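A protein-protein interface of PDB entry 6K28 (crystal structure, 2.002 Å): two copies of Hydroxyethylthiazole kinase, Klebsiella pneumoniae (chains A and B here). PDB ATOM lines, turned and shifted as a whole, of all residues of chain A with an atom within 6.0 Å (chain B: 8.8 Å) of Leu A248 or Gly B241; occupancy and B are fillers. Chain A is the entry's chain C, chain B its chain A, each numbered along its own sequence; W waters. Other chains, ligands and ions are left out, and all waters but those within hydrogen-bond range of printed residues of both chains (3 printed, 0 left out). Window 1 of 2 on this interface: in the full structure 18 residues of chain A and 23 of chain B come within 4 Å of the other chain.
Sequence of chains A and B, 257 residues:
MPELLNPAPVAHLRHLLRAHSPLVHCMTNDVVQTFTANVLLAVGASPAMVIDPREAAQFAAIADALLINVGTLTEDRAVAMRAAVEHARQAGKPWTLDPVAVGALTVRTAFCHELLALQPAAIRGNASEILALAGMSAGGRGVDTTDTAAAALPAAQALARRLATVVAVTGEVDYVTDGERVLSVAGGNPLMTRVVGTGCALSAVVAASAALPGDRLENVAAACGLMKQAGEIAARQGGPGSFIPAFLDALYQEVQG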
ATOM      1  N   PHE A  35     -23.818 -15.627 -19.239  1.00  0.00           N
ATOM      2  CA  PHE A  35     -24.456 -16.350 -18.156  1.00  0.00           C
ATOM      3  C   PHE A  35     -25.940 -15.967 -18.056  1.00  0.00           C
ATOM      4  O   PHE A  35     -26.812 -16.820 -17.800  1.00  0.00           O
ATOM      5  CB  PHE A  35     -23.704 -16.064 -16.842  1.00  0.00           C
ATOM      6  CG  PHE A  35     -24.205 -16.864 -15.665  1.00  0.00           C
ATOM      7  CD1 PHE A  35     -24.110 -18.253 -15.649  1.00  0.00           C
ATOM      8  CD2 PHE A  35     -24.781 -16.227 -14.572  1.00  0.00           C
ATOM      9  CE1 PHE A  35     -24.563 -18.975 -14.544  1.00  0.00           C
ATOM     10  CE2 PHE A  35     -25.241 -16.963 -13.469  1.00  0.00           C
ATOM     11  CZ  PHE A  35     -25.145 -18.322 -13.471  1.00  0.00           C
ATOM     12  N   ASN A  38     -27.666 -17.816 -20.774  1.00  0.00           N
ATOM     13  CA  ASN A  38     -27.797 -19.242 -20.510  1.00  0.00           C
ATOM     14  C   ASN A  38     -28.784 -19.545 -19.370  1.00  0.00           C
ATOM     15  O   ASN A  38     -29.448 -20.586 -19.385  1.00  0.00           O
ATOM     16  CB  ASN A  38     -26.430 -19.865 -20.192  1.00  0.00           C
ATOM     17  CG  ASN A  38     -25.634 -20.179 -21.439  1.00  0.00           C
ATOM     18  OD1 ASN A  38     -26.207 -20.462 -22.484  1.00  0.00           O
ATOM     19  ND2 ASN A  38     -24.313 -20.132 -21.340  1.00  0.00           N
ATOM     20  N   VAL A  39     -28.850 -18.675 -18.370  1.00  0.00           N
ATOM     21  CA  VAL A  39     -29.828 -18.831 -17.306  1.00  0.00           C
ATOM     22  C   VAL A  39     -31.259 -18.688 -17.868  1.00  0.00           C
ATOM     23  O   VAL A  39     -32.150 -19.503 -17.591  1.00  0.00           O
ATOM     24  CB  VAL A  39     -29.598 -17.786 -16.159  1.00  0.00           C
ATOM     25  CG1 VAL A  39     -30.817 -17.698 -15.247  1.00  0.00           C
ATOM     26  CG2 VAL A  39     -28.368 -18.178 -15.351  1.00  0.00           C
ATOM     27  N   ALA A  42     -31.930 -21.761 -19.694  1.00  0.00           N
ATOM     28  CA  ALA A  42     -32.108 -22.900 -18.793  1.00  0.00           C
ATOM     29  C   ALA A  42     -33.532 -22.931 -18.161  1.00  0.00           C
ATOM     30  O   ALA A  42     -34.065 -24.017 -17.894  1.00  0.00           O
ATOM     31  CB  ALA A  42     -31.094 -22.871 -17.717  1.00  0.00           C
ATOM     32  N   ALA A 234     -26.636 -26.295  -6.502  1.00  0.00           N
ATOM     33  CA  ALA A 234     -25.385 -26.094  -7.226  1.00  0.00           C
ATOM     34  C   ALA A 234     -24.206 -25.981  -6.265  1.00  0.00           C
ATOM     35  O   ALA A 234     -23.082 -26.402  -6.571  1.00  0.00           O
ATOM     36  CB  ALA A 234     -25.482 -24.828  -8.100  1.00  0.00           C
ATOM     37  N   PHE A 243     -19.933 -25.003  -9.597  1.00  0.00           N
ATOM     38  CA  PHE A 243     -21.225 -24.388  -9.353  1.00  0.00           C
ATOM     39  C   PHE A 243     -21.957 -23.992 -10.649  1.00  0.00           C
ATOM     40  O   PHE A 243     -23.168 -24.195 -10.800  1.00  0.00           O
ATOM     41  CB  PHE A 243     -21.040 -23.168  -8.464  1.00  0.00           C
ATOM     42  CG  PHE A 243     -22.288 -22.360  -8.254  1.00  0.00           C
ATOM     43  CD1 PHE A 243     -22.696 -21.424  -9.189  1.00  0.00           C
ATOM     44  CD2 PHE A 243     -23.041 -22.513  -7.094  1.00  0.00           C
ATOM     45  CE1 PHE A 243     -23.840 -20.669  -9.001  1.00  0.00           C
ATOM     46  CE2 PHE A 243     -24.192 -21.766  -6.895  1.00  0.00           C
ATOM     47  CZ  PHE A 243     -24.589 -20.834  -7.851  1.00  0.00           C
ATOM     48  N   ILE A 244     -21.231 -23.408 -11.586  1.00  0.00           N
ATOM     49  CA  ILE A 244     -21.873 -22.830 -12.749  1.00  0.00           C
ATOM     50  C   ILE A 244     -22.633 -23.892 -13.594  1.00  0.00           C
ATOM     51  O   ILE A 244     -23.831 -23.738 -13.867  1.00  0.00           O
ATOM     52  CB  ILE A 244     -20.825 -22.085 -13.604  1.00  0.00           C
ATOM     53  CG1 ILE A 244     -20.458 -20.772 -12.910  1.00  0.00           C
ATOM     54  CG2 ILE A 244     -21.346 -21.822 -15.029  1.00  0.00           C
ATOM     55  CD1 ILE A 244     -21.568 -19.735 -12.942  1.00  0.00           C
ATOM     56  N   PRO A 245     -21.947 -24.966 -14.003  1.00  0.00           N
ATOM     57  CA  PRO A 245     -22.718 -25.956 -14.771  1.00  0.00           C
ATOM     58  C   PRO A 245     -23.855 -26.576 -13.946  1.00  0.00           C
ATOM     59  O   PRO A 245     -24.952 -26.787 -14.460  1.00  0.00           O
ATOM     60  CB  PRO A 245     -21.687 -27.005 -15.147  1.00  0.00           C
ATOM     61  CG  PRO A 245     -20.372 -26.447 -14.818  1.00  0.00           C
ATOM     62  CD  PRO A 245     -20.518 -25.295 -13.936  1.00  0.00           C
ATOM     63  N   ALA A 246     -23.598 -26.841 -12.670  1.00  0.00           N
ATOM     64  CA  ALA A 246     -24.600 -27.447 -11.787  1.00  0.00           C
ATOM     65  C   ALA A 246     -25.821 -26.535 -11.620  1.00  0.00           C
ATOM     66  O   ALA A 246     -26.954 -27.002 -11.585  1.00  0.00           O
ATOM     67  CB  ALA A 246     -23.967 -27.774 -10.421  1.00  0.00           C
ATOM     68  N   PHE A 247     -25.586 -25.230 -11.527  1.00  0.00           N
ATOM     69  CA  PHE A 247     -26.645 -24.237 -11.409  1.00  0.00           C
ATOM     70  C   PHE A 247     -27.547 -24.196 -12.646  1.00  0.00           C
ATOM     71  O   PHE A 247     -28.796 -24.209 -12.538  1.00  0.00           O
ATOM     72  CB  PHE A 247     -26.021 -22.881 -11.175  1.00  0.00           C
ATOM     73  CG  PHE A 247     -26.979 -21.816 -10.820  1.00  0.00           C
ATOM     74  CD1 PHE A 247     -27.660 -21.842  -9.608  1.00  0.00           C
ATOM     75  CD2 PHE A 247     -27.174 -20.743 -11.667  1.00  0.00           C
ATOM     76  CE1 PHE A 247     -28.534 -20.834  -9.276  1.00  0.00           C
ATOM     77  CE2 PHE A 247     -28.072 -19.726 -11.338  1.00  0.00           C
ATOM     78  CZ  PHE A 247     -28.740 -19.771 -10.131  1.00  0.00           C
ATOM     79  N   LEU A 248     -26.921 -24.126 -13.824  1.00  0.00           N
ATOM     80  CA  LEU A 248     -27.708 -24.170 -15.064  1.00  0.00           C
ATOM     81  C   LEU A 248     -28.452 -25.516 -15.208  1.00  0.00           C
ATOM     82  O   LEU A 248     -29.634 -25.560 -15.573  1.00  0.00           O
ATOM     83  CB  LEU A 248     -26.805 -23.929 -16.271  1.00  0.00           C
ATOM     84  CG  LEU A 248     -26.153 -22.544 -16.299  1.00  0.00           C
ATOM     85  CD1 LEU A 248     -25.032 -22.496 -17.362  1.00  0.00           C
ATOM     86  CD2 LEU A 248     -27.193 -21.493 -16.575  1.00  0.00           C
ATOM     87  N   ASP A 249     -27.769 -26.608 -14.899  1.00  0.00           N
ATOM     88  CA  ASP A 249     -28.424 -27.914 -14.938  1.00  0.00           C
ATOM     89  C   ASP A 249     -29.630 -27.895 -13.987  1.00  0.00           C
ATOM     90  O   ASP A 249     -30.717 -28.362 -14.337  1.00  0.00           O
ATOM     91  CB  ASP A 249     -27.462 -29.044 -14.547  1.00  0.00           C
ATOM     92  CG  ASP A 249     -26.473 -29.403 -15.639  1.00  0.00           C
ATOM     93  OD1 ASP A 249     -26.532 -28.836 -16.760  1.00  0.00           O
ATOM     94  OD2 ASP A 249     -25.620 -30.282 -15.367  1.00  0.00           O
ATOM     95  N   ALA A 250     -29.454 -27.354 -12.788  1.00  0.00           N
ATOM     96  CA  ALA A 250     -30.537 -27.355 -11.803  1.00  0.00           C
ATOM     97  C   ALA A 250     -31.730 -26.566 -12.276  1.00  0.00           C
ATOM     98  O   ALA A 250     -32.869 -26.952 -12.019  1.00  0.00           O
ATOM     99  CB  ALA A 250     -30.071 -26.791 -10.457  1.00  0.00           C
ATOM    100  N   LEU A 251     -31.474 -25.420 -12.893  1.00  0.00           N
ATOM    101  CA  LEU A 251     -32.556 -24.610 -13.432  1.00  0.00           C
ATOM    102  C   LEU A 251     -33.302 -25.357 -14.516  1.00  0.00           C
ATOM    103  O   LEU A 251     -34.508 -25.226 -14.640  1.00  0.00           O
ATOM    104  CB  LEU A 251     -32.038 -23.296 -14.002  1.00  0.00           C
ATOM    105  CG  LEU A 251     -31.546 -22.257 -12.996  1.00  0.00           C
ATOM    106  CD1 LEU A 251     -30.863 -21.106 -13.750  1.00  0.00           C
ATOM    107  CD2 LEU A 251     -32.680 -21.746 -12.128  1.00  0.00           C
ATOM    108  N   TYR A 252     -32.561 -26.101 -15.320  1.00  0.00           N
ATOM    109  CA  TYR A 252     -33.148 -26.907 -16.373  1.00  0.00           C
ATOM    110  C   TYR A 252     -33.967 -28.116 -15.913  1.00  0.00           C
ATOM    111  O   TYR A 252     -34.950 -28.469 -16.561  1.00  0.00           O
ATOM    112  CB  TYR A 252     -32.032 -27.411 -17.285  1.00  0.00           C
ATOM    113  CG  TYR A 252     -32.514 -28.137 -18.516  1.00  0.00           C
ATOM    114  CD1 TYR A 252     -33.034 -27.432 -19.581  1.00  0.00           C
ATOM    115  CD2 TYR A 252     -32.419 -29.525 -18.624  1.00  0.00           C
ATOM    116  CE1 TYR A 252     -33.460 -28.061 -20.710  1.00  0.00           C
ATOM    117  CE2 TYR A 252     -32.852 -30.177 -19.773  1.00  0.00           C
ATOM    118  CZ  TYR A 252     -33.369 -29.420 -20.813  1.00  0.00           C
ATOM    119  OH  TYR A 252     -33.816 -30.006 -21.977  1.00  0.00           O
ATOM    120  N   GLN A 253     -33.529 -28.771 -14.837  1.00  0.00           N
ATOM    121  CA  GLN A 253     -34.077 -30.075 -14.430  1.00  0.00           C
ATOM    122  C   GLN A 253     -35.584 -30.051 -14.154  1.00  0.00           C
ATOM    123  O   GLN A 253     -36.087 -29.116 -13.530  1.00  0.00           O
ATOM    124  CB  GLN A 253     -33.355 -30.598 -13.177  1.00  0.00           C
ATOM    125  CG  GLN A 253     -31.983 -31.216 -13.431  1.00  0.00           C
ATOM    126  CD  GLN A 253     -31.973 -32.186 -14.600  1.00  0.00           C
ATOM    127  OE1 GLN A 253     -31.533 -31.841 -15.703  1.00  0.00           O
ATOM    128  NE2 GLN A 253     -32.455 -33.404 -14.368  1.00  0.00           N
ATOM    129  N   LEU B 191     -30.854 -30.112 -27.122  1.00  0.00           N
ATOM    130  CA  LEU B 191     -30.255 -29.384 -25.999  1.00  0.00           C
ATOM    131  C   LEU B 191     -29.269 -28.313 -26.491  1.00  0.00           C
ATOM    132  O   LEU B 191     -29.028 -27.311 -25.807  1.00  0.00           O
ATOM    133  CB  LEU B 191     -29.537 -30.340 -25.043  1.00  0.00           C
ATOM    134  CG  LEU B 191     -29.182 -29.802 -23.652  1.00  0.00           C
ATOM    135  CD1 LEU B 191     -30.438 -29.427 -22.860  1.00  0.00           C
ATOM    136  CD2 LEU B 191     -28.373 -30.810 -22.868  1.00  0.00           C
ATOM    137  N   ARG B 194     -30.523 -24.901 -26.194  1.00  0.00           N
ATOM    138  CA  ARG B 194     -30.717 -24.332 -24.877  1.00  0.00           C
ATOM    139  C   ARG B 194     -29.390 -23.848 -24.300  1.00  0.00           C
ATOM    140  O   ARG B 194     -29.279 -23.592 -23.112  1.00  0.00           O
ATOM    141  CB  ARG B 194     -31.369 -25.365 -23.954  1.00  0.00           C
ATOM    142  CG  ARG B 194     -32.643 -26.016 -24.572  1.00  0.00           C
ATOM    143  CD  ARG B 194     -33.621 -24.974 -25.136  1.00  0.00           C
ATOM    144  NE  ARG B 194     -34.102 -24.021 -24.128  1.00  0.00           N
ATOM    145  CZ  ARG B 194     -34.731 -22.877 -24.426  1.00  0.00           C
ATOM    146  NH1 ARG B 194     -34.934 -22.546 -25.696  1.00  0.00           N
ATOM    147  NH2 ARG B 194     -35.138 -22.043 -23.463  1.00  0.00           N
ATOM    148  N   VAL B 195     -28.388 -23.727 -25.152  1.00  0.00           N
ATOM    149  CA  VAL B 195     -27.082 -23.244 -24.739  1.00  0.00           C
ATOM    150  C   VAL B 195     -26.763 -22.108 -25.693  1.00  0.00           C
ATOM    151  O   VAL B 195     -26.886 -22.283 -26.890  1.00  0.00           O
ATOM    152  CB  VAL B 195     -26.047 -24.404 -24.772  1.00  0.00           C
ATOM    153  CG1 VAL B 195     -24.671 -23.918 -25.010  1.00  0.00           C
ATOM    154  CG2 VAL B 195     -26.119 -25.190 -23.453  1.00  0.00           C
ATOM    155  N   VAL B 196     -26.411 -20.924 -25.197  1.00  0.00           N
ATOM    156  CA  VAL B 196     -26.257 -19.809 -26.128  1.00  0.00           C
ATOM    157  C   VAL B 196     -24.967 -19.983 -26.949  1.00  0.00           C
ATOM    158  O   VAL B 196     -23.957 -20.477 -26.452  1.00  0.00           O
ATOM    159  CB  VAL B 196     -26.270 -18.463 -25.398  1.00  0.00           C
ATOM    160  CG1 VAL B 196     -24.955 -18.214 -24.675  1.00  0.00           C
ATOM    161  CG2 VAL B 196     -26.612 -17.347 -26.379  1.00  0.00           C
ATOM    162  N   ALA B 234     -22.026 -34.209 -26.116  1.00  0.00           N
ATOM    163  CA  ALA B 234     -22.226 -33.363 -24.959  1.00  0.00           C
ATOM    164  C   ALA B 234     -23.627 -33.455 -24.395  1.00  0.00           C
ATOM    165  O   ALA B 234     -23.786 -33.298 -23.199  1.00  0.00           O
ATOM    166  CB  ALA B 234     -21.896 -31.902 -25.305  1.00  0.00           C
ATOM    167  N   GLN B 237     -24.788 -35.639 -21.250  1.00  0.00           N
ATOM    168  CA  GLN B 237     -24.670 -35.214 -19.848  1.00  0.00           C
ATOM    169  C   GLN B 237     -25.973 -34.695 -19.251  1.00  0.00           C
ATOM    170  O   GLN B 237     -25.997 -34.255 -18.098  1.00  0.00           O
ATOM    171  CB  GLN B 237     -23.670 -34.099 -19.699  1.00  0.00           C
ATOM    172  CG  GLN B 237     -22.283 -34.342 -20.219  1.00  0.00           C
ATOM    173  CD  GLN B 237     -21.585 -35.434 -19.486  1.00  0.00           C
ATOM    174  OE1 GLN B 237     -21.527 -35.418 -18.249  1.00  0.00           O
ATOM    175  NE2 GLN B 237     -21.055 -36.402 -20.227  1.00  0.00           N
ATOM    176  N   GLY B 238     -27.042 -34.674 -20.035  1.00  0.00           N
ATOM    177  CA  GLY B 238     -28.355 -34.340 -19.509  1.00  0.00           C
ATOM    178  C   GLY B 238     -28.780 -32.873 -19.426  1.00  0.00           C
ATOM    179  O   GLY B 238     -29.971 -32.574 -19.653  1.00  0.00           O
ATOM    180  N   GLY B 239     -27.854 -31.966 -19.082  1.00  0.00           N
ATOM    181  CA  GLY B 239     -28.202 -30.569 -18.842  1.00  0.00           C
ATOM    182  C   GLY B 239     -27.340 -29.570 -19.595  1.00  0.00           C
ATOM    183  O   GLY B 239     -26.222 -29.883 -19.977  1.00  0.00           O
ATOM    184  N   PRO B 240     -27.855 -28.350 -19.794  1.00  0.00           N
ATOM    185  CA  PRO B 240     -27.173 -27.339 -20.610  1.00  0.00           C
ATOM    186  C   PRO B 240     -25.919 -26.773 -19.964  1.00  0.00           C
ATOM    187  O   PRO B 240     -25.042 -26.304 -20.667  1.00  0.00           O
ATOM    188  CB  PRO B 240     -28.229 -26.256 -20.769  1.00  0.00           C
ATOM    189  CG  PRO B 240     -29.079 -26.384 -19.533  1.00  0.00           C
ATOM    190  CD  PRO B 240     -29.100 -27.838 -19.194  1.00  0.00           C
ATOM    191  N   GLY B 241     -25.844 -26.809 -18.645  1.00  0.00           N
ATOM    192  CA  GLY B 241     -24.655 -26.378 -17.925  1.00  0.00           C
ATOM    193  C   GLY B 241     -23.509 -27.338 -18.123  1.00  0.00           C
ATOM    194  O   GLY B 241     -22.418 -26.938 -18.517  1.00  0.00           O
ATOM    195  N   SER B 242     -23.769 -28.624 -17.893  1.00  0.00           N
ATOM    196  CA  SER B 242     -22.773 -29.671 -18.130  1.00  0.00           C
ATOM    197  C   SER B 242     -22.487 -29.877 -19.611  1.00  0.00           C
ATOM    198  O   SER B 242     -21.417 -30.351 -19.997  1.00  0.00           O
ATOM    199  CB  SER B 242     -23.244 -31.004 -17.524  1.00  0.00           C
ATOM    200  OG  SER B 242     -23.313 -30.899 -16.125  1.00  0.00           O
ATOM    201  N   PHE B 243     -23.453 -29.529 -20.441  1.00  0.00           N
ATOM    202  CA  PHE B 243     -23.249 -29.582 -21.890  1.00  0.00           C
ATOM    203  C   PHE B 243     -21.951 -28.877 -22.337  1.00  0.00           C
ATOM    204  O   PHE B 243     -21.183 -29.369 -23.186  1.00  0.00           O
ATOM    205  CB  PHE B 243     -24.443 -28.946 -22.606  1.00  0.00           C
ATOM    206  CG  PHE B 243     -24.293 -28.867 -24.094  1.00  0.00           C
ATOM    207  CD1 PHE B 243     -23.587 -27.836 -24.693  1.00  0.00           C
ATOM    208  CD2 PHE B 243     -24.876 -29.819 -24.905  1.00  0.00           C
ATOM    209  CE1 PHE B 243     -23.459 -27.782 -26.062  1.00  0.00           C
ATOM    210  CE2 PHE B 243     -24.754 -29.751 -26.269  1.00  0.00           C
ATOM    211  CZ  PHE B 243     -24.045 -28.741 -26.847  1.00  0.00           C
ATOM    212  N   ILE B 244     -21.707 -27.707 -21.775  1.00  0.00           N
ATOM    213  CA  ILE B 244     -20.678 -26.815 -22.333  1.00  0.00           C
ATOM    214  C   ILE B 244     -19.267 -27.404 -22.170  1.00  0.00           C
ATOM    215  O   ILE B 244     -18.539 -27.608 -23.166  1.00  0.00           O
ATOM    216  CB  ILE B 244     -20.784 -25.405 -21.703  1.00  0.00           C
ATOM    217  CG1 ILE B 244     -22.041 -24.696 -22.237  1.00  0.00           C
ATOM    218  CG2 ILE B 244     -19.550 -24.549 -22.040  1.00  0.00           C
ATOM    219  CD1 ILE B 244     -22.605 -23.594 -21.283  1.00  0.00           C
ATOM    220  N   PRO B 245     -18.877 -27.746 -20.930  1.00  0.00           N
ATOM    221  CA  PRO B 245     -17.563 -28.399 -20.811  1.00  0.00           C
ATOM    222  C   PRO B 245     -17.392 -29.687 -21.645  1.00  0.00           C
ATOM    223  O   PRO B 245     -16.318 -29.946 -22.233  1.00  0.00           O
ATOM    224  CB  PRO B 245     -17.450 -28.709 -19.313  1.00  0.00           C
ATOM    225  CG  PRO B 245     -18.721 -28.307 -18.696  1.00  0.00           C
ATOM    226  CD  PRO B 245     -19.423 -27.372 -19.621  1.00  0.00           C
ATOM    227  N   ALA B 246     -18.455 -30.480 -21.702  1.00  0.00           N
ATOM    228  CA  ALA B 246     -18.443 -31.732 -22.453  1.00  0.00           C
ATOM    229  C   ALA B 246     -18.286 -31.478 -23.948  1.00  0.00           C
ATOM    230  O   ALA B 246     -17.578 -32.198 -24.659  1.00  0.00           O
ATOM    231  CB  ALA B 246     -19.742 -32.523 -22.173  1.00  0.00           C
ATOM    232  N   PHE B 247     -18.955 -30.426 -24.430  1.00  0.00           N
ATOM    233  CA  PHE B 247     -18.899 -30.047 -25.848  1.00  0.00           C
ATOM    234  C   PHE B 247     -17.482 -29.636 -26.246  1.00  0.00           C
ATOM    235  O   PHE B 247     -16.891 -30.103 -27.268  1.00  0.00           O
ATOM    236  CB  PHE B 247     -19.923 -28.915 -26.085  1.00  0.00           C
ATOM    237  CG  PHE B 247     -20.059 -28.485 -27.524  1.00  0.00           C
ATOM    238  CD1 PHE B 247     -20.832 -29.234 -28.425  1.00  0.00           C
ATOM    239  CD2 PHE B 247     -19.459 -27.323 -27.974  1.00  0.00           C
ATOM    240  CE1 PHE B 247     -20.990 -28.828 -29.755  1.00  0.00           C
ATOM    241  CE2 PHE B 247     -19.623 -26.897 -29.332  1.00  0.00           C
ATOM    242  CZ  PHE B 247     -20.384 -27.661 -30.206  1.00  0.00           C
ATOM    243  N   LEU B 248     -16.890 -28.771 -25.423  1.00  0.00           N
ATOM    244  CA  LEU B 248     -15.511 -28.372 -25.685  1.00  0.00           C
ATOM    245  C   LEU B 248     -14.535 -29.528 -25.577  1.00  0.00           C
ATOM    246  O   LEU B 248     -13.645 -29.648 -26.401  1.00  0.00           O
ATOM    247  CB  LEU B 248     -15.071 -27.262 -24.742  1.00  0.00           C
ATOM    248  CG  LEU B 248     -15.816 -25.941 -24.957  1.00  0.00           C
ATOM    249  CD1 LEU B 248     -15.678 -25.043 -23.736  1.00  0.00           C
ATOM    250  CD2 LEU B 248     -15.362 -25.233 -26.246  1.00  0.00           C
HETATM  251  O   HOH W   1     -33.525 -29.830 -24.943  1.00  0.00           O
HETATM  252  O   HOH W   2     -28.008 -32.439 -16.617  1.00  0.00           O
HETATM  253  O   HOH W   3     -28.496 -22.891 -20.559  1.00  0.00           O
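Water W2 lies within hydrogen-bond range of the backbone NH of Gly B239 (2.5 Å), the backbone carbonyl oxygen of Gln B237 (3.1 Å) and the side-chain carboxylate of Asp A249 (3.5 Å).
Water W3 bridges the backbone carbonyl oxygen (O) of Asn A38 and the backbone carbonyl oxygen (O) of Arg B194.
Water W1 lies within hydrogen-bond range of OH of Tyr A252 (3.0 Å) and N of Leu B191 (3.5 Å).
Printed residues of chain B that touch a printed residue of chain A: Leu B191, Val B195, Val B196, Gly B238, Gly B239, Pro B240, Gly B241, Ser B242 and Ile B244.
Hydrophobic or aromatic side chains of chain B that line the printed part of chain A: Leu B191, Val B196, Pro B240 and Ile B244.
Printed residues of chain A that touch a printed residue of chain B: Asn A38, Pro A245, Leu A248, Asp A249 and Tyr A252.
Hydrophobic or aromatic side chains of chain A that line the printed part of chain B: Pro A245, Leu A248 and Tyr A252.
The backbone NH of Val B196 sits at hydrogen-bond distance from the side-chain amide oxygen of Asn A38 (2.8 Å).
The backbone NH of Gly B241 is in hydrogen-bond range of the side-chain carboxylate of Asp A249, at 2.9 Å.
The side-chain carboxylate of Asp A249 sits at hydrogen-bond distance from the side-chain hydroxyl of Ser B242, at 2.5 Å.
The backbone carbonyl oxygen (O) of Gly B239 lies close to the side-chain carboxylate (OD1) of Asp A249 (3.4 Å).
The backbone nitrogen of Pro B240 lies close to the side-chain carboxylate of Asp A249.
Positions printed for both chains: 234, 243, 244, 245, 246, 247 and 248.
Of the 13 pairs that touch across the chains among the printed residues, none has its exchanged pair printed and touching as well.
Of the printed residues of chain B, Asn A38 touches Val B195 (3.6 Å), Val B196 (2.8 Å) and Ile B244 (3.9 Å).
Of chain B, only Gly B241 comes within 4 Å of Leu A248.
Of chain B, only Gly B239 (3.0 Å), Pro B240 (3.3 Å), Gly B241 (2.9 Å) and Ser B242 (2.5 Å) come within 4 Å of Asp A249.
Printed residues of chain A within 4 Å of Gly B239: Asp A249 (3.0 Å).
Of the printed residues of chain A, Pro B240 touches Asp A249 (3.3 Å) and Tyr A252 (3.5 Å).
Gly B241 touches just these residues of chain A: Pro A245 (3.4 Å), Leu A248 (3.7 Å) and Asp A249 (2.9 Å).
The nearest residue of chain B that does not touch Leu A248 is Pro B240 (4.1 Å).
The nearest printed residue of chain A that does not touch Val B196 is Phe A35 (6.1 Å).
Val B195 touches Asn A38 (C to OD1, 3.6 Å).
Ile B244 touches Asn A38 (CD1 to ND2, 3.9 Å).
Pro A245 touches Gly B241 (CB to O, 3.4 Å).
CB of Pro A245 touches N of Ser B242 (3.8 Å).
Leu A248 touches Gly B241 (CB to CA, 3.7 Å).
Tyr A252 touches Leu B191 (OH to CD1, 3.5 Å).
Tyr A252 touches Gly B238 (CE2 to O, 3.7 Å).
Tyr A252 touches Pro B240 (CG to CD, 3.5 Å).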
